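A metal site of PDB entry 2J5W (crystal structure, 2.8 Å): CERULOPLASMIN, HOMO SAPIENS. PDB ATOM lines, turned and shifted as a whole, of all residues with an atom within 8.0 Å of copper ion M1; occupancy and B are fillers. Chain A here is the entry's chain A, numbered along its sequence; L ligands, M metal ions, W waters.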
ATOM      1  N   HIS A 120      18.273 -15.207  24.870  1.00  0.00           N
ATOM      2  CA  HIS A 120      17.683 -14.822  23.580  1.00  0.00           C
ATOM      3  C   HIS A 120      16.697 -13.718  23.820  1.00  0.00           C
ATOM      4  O   HIS A 120      15.770 -13.898  24.605  1.00  0.00           O
ATOM      5  CB  HIS A 120      16.963 -16.008  22.945  1.00  0.00           C
ATOM      6  CG  HIS A 120      16.111 -15.654  21.759  1.00  0.00           C
ATOM      7  ND1 HIS A 120      16.614 -15.032  20.646  1.00  0.00           N
ATOM      8  CD2 HIS A 120      14.797 -15.860  21.518  1.00  0.00           C
ATOM      9  CE1 HIS A 120      15.633 -14.848  19.768  1.00  0.00           C
ATOM     10  NE2 HIS A 120      14.521 -15.337  20.278  1.00  0.00           N
ATOM     11  N   HIS A 122      13.746 -10.891  22.543  1.00  0.00           N
ATOM     12  CA  HIS A 122      12.735 -10.508  21.552  1.00  0.00           C
ATOM     13  C   HIS A 122      12.850  -9.005  21.282  1.00  0.00           C
ATOM     14  O   HIS A 122      13.380  -8.270  22.108  1.00  0.00           O
ATOM     15  CB  HIS A 122      11.321 -10.827  22.048  1.00  0.00           C
ATOM     16  CG  HIS A 122      10.946 -12.275  21.955  1.00  0.00           C
ATOM     17  ND1 HIS A 122       9.797 -12.709  21.334  1.00  0.00           N
ATOM     18  CD2 HIS A 122      11.566 -13.394  22.428  1.00  0.00           C
ATOM     19  CE1 HIS A 122       9.722 -14.027  21.416  1.00  0.00           C
ATOM     20  NE2 HIS A 122      10.782 -14.463  22.068  1.00  0.00           N
ATOM     21  N   TYR A 126      20.060  -7.967  16.721  1.00  0.00           N
ATOM     22  CA  TYR A 126      21.291  -8.649  17.031  1.00  0.00           C
ATOM     23  C   TYR A 126      21.773  -9.282  15.742  1.00  0.00           C
ATOM     24  O   TYR A 126      21.001  -9.480  14.799  1.00  0.00           O
ATOM     25  CB  TYR A 126      21.093  -9.711  18.113  1.00  0.00           C
ATOM     26  CG  TYR A 126      19.804 -10.496  17.985  1.00  0.00           C
ATOM     27  CD1 TYR A 126      19.627 -11.405  16.961  1.00  0.00           C
ATOM     28  CD2 TYR A 126      18.775 -10.323  18.904  1.00  0.00           C
ATOM     29  CE1 TYR A 126      18.446 -12.124  16.845  1.00  0.00           C
ATOM     30  CE2 TYR A 126      17.594 -11.033  18.792  1.00  0.00           C
ATOM     31  CZ  TYR A 126      17.429 -11.935  17.754  1.00  0.00           C
ATOM     32  OH  TYR A 126      16.249 -12.638  17.606  1.00  0.00           O
ATOM     33  N   GLU A 131      22.210 -13.831  19.036  1.00  0.00           N
ATOM     34  CA  GLU A 131      20.819 -14.273  19.037  1.00  0.00           C
ATOM     35  C   GLU A 131      20.522 -15.207  20.192  1.00  0.00           C
ATOM     36  O   GLU A 131      19.391 -15.305  20.632  1.00  0.00           O
ATOM     37  CB  GLU A 131      20.465 -14.968  17.721  1.00  0.00           C
ATOM     38  CG  GLU A 131      19.115 -15.704  17.667  1.00  0.00           C
ATOM     39  CD  GLU A 131      18.779 -16.247  16.293  1.00  0.00           C
ATOM     40  OE1 GLU A 131      19.696 -16.303  15.443  1.00  0.00           O
ATOM     41  OE2 GLU A 131      17.607 -16.622  16.048  1.00  0.00           O
ATOM     42  N   ALA A 133      20.201 -18.424  20.336  1.00  0.00           N
ATOM     43  CA  ALA A 133      19.238 -19.468  19.998  1.00  0.00           C
ATOM     44  C   ALA A 133      19.915 -20.475  19.057  1.00  0.00           C
ATOM     45  O   ALA A 133      20.549 -20.089  18.075  1.00  0.00           O
ATOM     46  CB  ALA A 133      17.998 -18.874  19.368  1.00  0.00           C
ATOM     47  N   ILE A 134      19.805 -21.755  19.395  1.00  0.00           N
ATOM     48  CA  ILE A 134      20.458 -22.801  18.622  1.00  0.00           C
ATOM     49  C   ILE A 134      19.442 -23.480  17.698  1.00  0.00           C
ATOM     50  O   ILE A 134      18.391 -23.954  18.139  1.00  0.00           O
ATOM     51  CB  ILE A 134      21.148 -23.847  19.541  1.00  0.00           C
ATOM     52  CG1 ILE A 134      22.278 -24.546  18.770  1.00  0.00           C
ATOM     53  CG2 ILE A 134      20.163 -24.866  20.119  1.00  0.00           C
ATOM     54  CD1 ILE A 134      23.330 -25.189  19.682  1.00  0.00           C
ATOM     55  N   TYR A 135      19.763 -23.468  16.402  1.00  0.00           N
ATOM     56  CA  TYR A 135      18.988 -24.157  15.388  1.00  0.00           C
ATOM     57  C   TYR A 135      19.814 -24.168  14.099  1.00  0.00           C
ATOM     58  O   TYR A 135      20.766 -23.402  13.985  1.00  0.00           O
ATOM     59  CB  TYR A 135      17.634 -23.490  15.165  1.00  0.00           C
ATOM     60  CG  TYR A 135      17.659 -22.005  14.854  1.00  0.00           C
ATOM     61  CD1 TYR A 135      17.716 -21.063  15.868  1.00  0.00           C
ATOM     62  CD2 TYR A 135      17.610 -21.546  13.540  1.00  0.00           C
ATOM     63  CE1 TYR A 135      17.735 -19.680  15.581  1.00  0.00           C
ATOM     64  CE2 TYR A 135      17.622 -20.187  13.235  1.00  0.00           C
ATOM     65  CZ  TYR A 135      17.682 -19.260  14.256  1.00  0.00           C
ATOM     66  OH  TYR A 135      17.673 -17.919  13.938  1.00  0.00           O
ATOM     67  N   HIS A 180      14.600 -14.964  27.060  1.00  0.00           N
ATOM     68  CA  HIS A 180      14.639 -16.273  27.699  1.00  0.00           C
ATOM     69  C   HIS A 180      15.716 -17.143  27.086  1.00  0.00           C
ATOM     70  O   HIS A 180      16.326 -16.768  26.079  1.00  0.00           O
ATOM     71  CB  HIS A 180      13.281 -16.951  27.571  1.00  0.00           C
ATOM     72  CG  HIS A 180      12.822 -17.100  26.157  1.00  0.00           C
ATOM     73  ND1 HIS A 180      13.182 -18.167  25.372  1.00  0.00           N
ATOM     74  CD2 HIS A 180      12.031 -16.315  25.393  1.00  0.00           C
ATOM     75  CE1 HIS A 180      12.614 -18.043  24.183  1.00  0.00           C
ATOM     76  NE2 HIS A 180      11.909 -16.923  24.172  1.00  0.00           N
ATOM     77  N   SER A 181      15.956 -18.301  27.689  1.00  0.00           N
ATOM     78  CA  SER A 181      16.933 -19.232  27.144  1.00  0.00           C
ATOM     79  C   SER A 181      16.324 -20.038  25.980  1.00  0.00           C
ATOM     80  O   SER A 181      15.121 -20.276  25.950  1.00  0.00           O
ATOM     81  CB  SER A 181      17.473 -20.156  28.230  1.00  0.00           C
ATOM     82  OG  SER A 181      18.359 -21.111  27.681  1.00  0.00           O
ATOM     83  N   HIS A 182      17.153 -20.405  25.003  1.00  0.00           N
ATOM     84  CA  HIS A 182      16.661 -20.950  23.753  1.00  0.00           C
ATOM     85  C   HIS A 182      17.579 -22.051  23.208  1.00  0.00           C
ATOM     86  O   HIS A 182      18.091 -21.940  22.091  1.00  0.00           O
ATOM     87  CB  HIS A 182      16.507 -19.814  22.731  1.00  0.00           C
ATOM     88  CG  HIS A 182      15.531 -20.102  21.632  1.00  0.00           C
ATOM     89  ND1 HIS A 182      15.620 -21.208  20.830  1.00  0.00           N
ATOM     90  CD2 HIS A 182      14.453 -19.393  21.194  1.00  0.00           C
ATOM     91  CE1 HIS A 182      14.623 -21.190  19.946  1.00  0.00           C
ATOM     92  NE2 HIS A 182      13.899 -20.102  20.155  1.00  0.00           N
ATOM     93  N   ALA A 185      13.776 -24.030  24.165  1.00  0.00           N
ATOM     94  CA  ALA A 185      13.123 -22.873  24.760  1.00  0.00           C
ATOM     95  C   ALA A 185      11.990 -23.280  25.688  1.00  0.00           C
ATOM     96  O   ALA A 185      11.959 -22.858  26.839  1.00  0.00           O
ATOM     97  CB  ALA A 185      12.637 -21.916  23.681  1.00  0.00           C
ATOM     98  N   PRO A 186      11.038 -24.086  25.208  1.00  0.00           N
ATOM     99  CA  PRO A 186       9.978 -24.538  26.100  1.00  0.00           C
ATOM    100  C   PRO A 186      10.463 -25.118  27.410  1.00  0.00           C
ATOM    101  O   PRO A 186       9.863 -24.858  28.444  1.00  0.00           O
ATOM    102  CB  PRO A 186       9.272 -25.612  25.285  1.00  0.00           C
ATOM    103  CG  PRO A 186       9.438 -25.121  23.883  1.00  0.00           C
ATOM    104  CD  PRO A 186      10.823 -24.555  23.832  1.00  0.00           C
ATOM    105  N   ILE A 189      12.494 -22.338  29.520  1.00  0.00           N
ATOM    106  CA  ILE A 189      11.537 -21.373  30.086  1.00  0.00           C
ATOM    107  C   ILE A 189      10.753 -22.000  31.248  1.00  0.00           C
ATOM    108  O   ILE A 189      10.521 -21.352  32.260  1.00  0.00           O
ATOM    109  CB  ILE A 189      10.539 -20.816  29.018  1.00  0.00           C
ATOM    110  CG1 ILE A 189      11.260 -19.940  27.980  1.00  0.00           C
ATOM    111  CG2 ILE A 189       9.451 -19.989  29.669  1.00  0.00           C
ATOM    112  CD1 ILE A 189      10.480 -19.728  26.681  1.00  0.00           C
ATOM    113  N   HIS A 997       6.071 -16.051  15.788  1.00  0.00           N
ATOM    114  CA  HIS A 997       7.244 -15.270  16.183  1.00  0.00           C
ATOM    115  C   HIS A 997       8.357 -15.361  15.153  1.00  0.00           C
ATOM    116  O   HIS A 997       8.671 -16.446  14.670  1.00  0.00           O
ATOM    117  CB  HIS A 997       7.752 -15.748  17.538  1.00  0.00           C
ATOM    118  CG  HIS A 997       9.048 -15.130  17.959  1.00  0.00           C
ATOM    119  ND1 HIS A 997       9.289 -13.775  17.865  1.00  0.00           N
ATOM    120  CD2 HIS A 997      10.174 -15.689  18.460  1.00  0.00           C
ATOM    121  CE1 HIS A 997      10.514 -13.532  18.291  1.00  0.00           C
ATOM    122  NE2 HIS A 997      11.073 -14.670  18.663  1.00  0.00           N
ATOM    123  N   PHE A 998       8.942 -14.198  14.829  1.00  0.00           N
ATOM    124  CA  PHE A 998      10.048 -14.091  13.873  1.00  0.00           C
ATOM    125  C   PHE A 998      11.333 -13.767  14.615  1.00  0.00           C
ATOM    126  O   PHE A 998      11.461 -12.691  15.186  1.00  0.00           O
ATOM    127  CB  PHE A 998       9.825 -12.943  12.886  1.00  0.00           C
ATOM    128  CG  PHE A 998       8.638 -13.089  11.998  1.00  0.00           C
ATOM    129  CD1 PHE A 998       7.389 -12.647  12.395  1.00  0.00           C
ATOM    130  CD2 PHE A 998       8.771 -13.612  10.722  1.00  0.00           C
ATOM    131  CE1 PHE A 998       6.303 -12.746  11.558  1.00  0.00           C
ATOM    132  CE2 PHE A 998       7.670 -13.716   9.870  1.00  0.00           C
ATOM    133  CZ  PHE A 998       6.439 -13.266  10.300  1.00  0.00           C
ATOM    134  N   HIS A 999      12.291 -14.676  14.610  1.00  0.00           N
ATOM    135  CA  HIS A 999      13.632 -14.364  15.112  1.00  0.00           C
ATOM    136  C   HIS A 999      14.269 -13.300  14.205  1.00  0.00           C
ATOM    137  O   HIS A 999      14.024 -13.278  12.986  1.00  0.00           O
ATOM    138  CB  HIS A 999      14.521 -15.606  15.165  1.00  0.00           C
ATOM    139  CG  HIS A 999      14.244 -16.526  16.315  1.00  0.00           C
ATOM    140  ND1 HIS A 999      15.235 -16.963  17.164  1.00  0.00           N
ATOM    141  CD2 HIS A 999      13.096 -17.102  16.748  1.00  0.00           C
ATOM    142  CE1 HIS A 999      14.720 -17.773  18.068  1.00  0.00           C
ATOM    143  NE2 HIS A 999      13.411 -17.875  17.845  1.00  0.00           N
ATOM    144  N   LEU A1037      15.012 -18.142  12.510  1.00  0.00           N
ATOM    145  CA  LEU A1037      13.953 -19.056  12.891  1.00  0.00           C
ATOM    146  C   LEU A1037      12.609 -18.302  12.875  1.00  0.00           C
ATOM    147  O   LEU A1037      12.542 -17.134  13.240  1.00  0.00           O
ATOM    148  CB  LEU A1037      14.265 -19.675  14.262  1.00  0.00           C
ATOM    149  CG  LEU A1037      13.464 -20.925  14.670  1.00  0.00           C
ATOM    150  CD1 LEU A1037      13.809 -22.125  13.815  1.00  0.00           C
ATOM    151  CD2 LEU A1037      13.710 -21.238  16.138  1.00  0.00           C
ATOM    152  N   LEU A1038      11.570 -18.969  12.399  1.00  0.00           N
ATOM    153  CA  LEU A1038      10.219 -18.437  12.357  1.00  0.00           C
ATOM    154  C   LEU A1038       9.327 -19.553  12.847  1.00  0.00           C
ATOM    155  O   LEU A1038       9.224 -20.581  12.183  1.00  0.00           O
ATOM    156  CB  LEU A1038       9.865 -18.088  10.918  1.00  0.00           C
ATOM    157  CG  LEU A1038       8.524 -17.471  10.525  1.00  0.00           C
ATOM    158  CD1 LEU A1038       8.472 -17.451   9.014  1.00  0.00           C
ATOM    159  CD2 LEU A1038       7.373 -18.229  11.054  1.00  0.00           C
ATOM    160  N   HIS A1039       8.692 -19.372  13.993  1.00  0.00           N
ATOM    161  CA  HIS A1039       7.949 -20.471  14.599  1.00  0.00           C
ATOM    162  C   HIS A1039       6.776 -20.011  15.486  1.00  0.00           C
ATOM    163  O   HIS A1039       6.786 -18.930  16.033  1.00  0.00           O
ATOM    164  CB  HIS A1039       8.920 -21.319  15.419  1.00  0.00           C
ATOM    165  CG  HIS A1039       9.505 -20.592  16.605  1.00  0.00           C
ATOM    166  ND1 HIS A1039       8.867 -20.550  17.827  1.00  0.00           N
ATOM    167  CD2 HIS A1039      10.657 -19.902  16.753  1.00  0.00           C
ATOM    168  CE1 HIS A1039       9.611 -19.845  18.670  1.00  0.00           C
ATOM    169  NE2 HIS A1039      10.699 -19.456  18.045  1.00  0.00           N
ATOM    170  N   CYS A1040       5.756 -20.854  15.614  1.00  0.00           N
ATOM    171  CA  CYS A1040       4.725 -20.650  16.605  1.00  0.00           C
ATOM    172  C   CYS A1040       5.403 -20.866  17.945  1.00  0.00           C
ATOM    173  O   CYS A1040       6.267 -21.712  18.052  1.00  0.00           O
ATOM    174  CB  CYS A1040       3.601 -21.645  16.399  1.00  0.00           C
ATOM    175  SG  CYS A1040       2.417 -21.675  17.711  1.00  0.00           S
ATOM    176  N   HIS A1041       5.006 -20.093  18.960  1.00  0.00           N
ATOM    177  CA  HIS A1041       5.690 -20.049  20.250  1.00  0.00           C
ATOM    178  C   HIS A1041       4.960 -20.896  21.295  1.00  0.00           C
ATOM    179  O   HIS A1041       5.320 -20.862  22.457  1.00  0.00           O
ATOM    180  CB  HIS A1041       5.760 -18.589  20.716  1.00  0.00           C
ATOM    181  CG  HIS A1041       6.939 -18.265  21.581  1.00  0.00           C
ATOM    182  ND1 HIS A1041       7.072 -18.732  22.875  1.00  0.00           N
ATOM    183  CD2 HIS A1041       8.009 -17.454  21.364  1.00  0.00           C
ATOM    184  CE1 HIS A1041       8.180 -18.240  23.397  1.00  0.00           C
ATOM    185  NE2 HIS A1041       8.774 -17.467  22.508  1.00  0.00           N
ATOM    186  N   ILE A1046       5.811 -26.110  18.874  1.00  0.00           N
ATOM    187  CA  ILE A1046       7.229 -26.000  18.507  1.00  0.00           C
ATOM    188  C   ILE A1046       7.810 -27.401  18.420  1.00  0.00           C
ATOM    189  O   ILE A1046       8.369 -27.782  17.398  1.00  0.00           O
ATOM    190  CB  ILE A1046       8.070 -25.222  19.551  1.00  0.00           C
ATOM    191  CG1 ILE A1046       7.566 -23.806  19.751  1.00  0.00           C
ATOM    192  CG2 ILE A1046       9.534 -25.145  19.120  1.00  0.00           C
ATOM    193  CD1 ILE A1046       8.307 -23.072  20.872  1.00  0.00           C
ATOM    194  N   GLU A1051       7.482 -24.909  12.615  1.00  0.00           N
ATOM    195  CA  GLU A1051       8.598 -23.971  12.531  1.00  0.00           C
ATOM    196  C   GLU A1051       9.343 -24.118  11.214  1.00  0.00           C
ATOM    197  O   GLU A1051       9.292 -25.174  10.590  1.00  0.00           O
ATOM    198  CB  GLU A1051       9.591 -24.220  13.677  1.00  0.00           C
ATOM    199  CG  GLU A1051      10.182 -25.620  13.724  1.00  0.00           C
ATOM    200  CD  GLU A1051      11.057 -25.863  14.959  1.00  0.00           C
ATOM    201  OE1 GLU A1051      11.600 -24.865  15.504  1.00  0.00           O
ATOM    202  OE2 GLU A1051      11.204 -27.046  15.377  1.00  0.00           O
HETATM  203  O1  LIG L   1      11.600 -17.698  21.173  1.00  0.00           O
HETATM  204  O2  LIG L   1      12.010 -16.836  20.672  1.00  0.00           O
HETATM  205 CU    CU M   1      12.404 -19.055  19.058  1.00  0.00          CU
HETATM  206 CU    CU M   2      12.830 -15.081  19.518  1.00  0.00          CU
HETATM  207 CU    CU M   3      10.583 -16.240  22.724  1.00  0.00          CU
HETATM  208  O   HOH W   1      11.153 -20.086  21.075  1.00  0.00           O
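Leu 1037 touches copper ion M1. Within 4 Å of copper ion M1: His 182, His 999, Leu 1037 and His 1039. The nearest printed residue that does not touch copper ion M1 is His 997 (4.1 Å).
Copper ion M1 is bound by a ring nitrogen (NE2) of His 999, a ring nitrogen (NE2) of His 1039, a ring nitrogen (NE2) of His 182 and water W1. Copper ion M1 has four donor atoms within binding distance. Slightly farther from copper ion M1 lies an oxygen (O1) of the ligand (2.6 Å).
The backbone NH (N) of His 999 sits at hydrogen-bond distance from the backbone carbonyl oxygen (O) of Leu 1037, 2.8 Å away. OE2 of Glu 131 sits at hydrogen-bond distance from ND1 of His 999 (2.6 Å). O of His 1039 lies within hydrogen-bond range of N of His 997, at 3.0 Å. The backbone carbonyl oxygen of His 182 sits at hydrogen-bond distance from the backbone NH of Ile 134 (3.2 Å). N of Leu 1037 sits at hydrogen-bond distance from OH of Tyr 135, at 3.0 Å.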
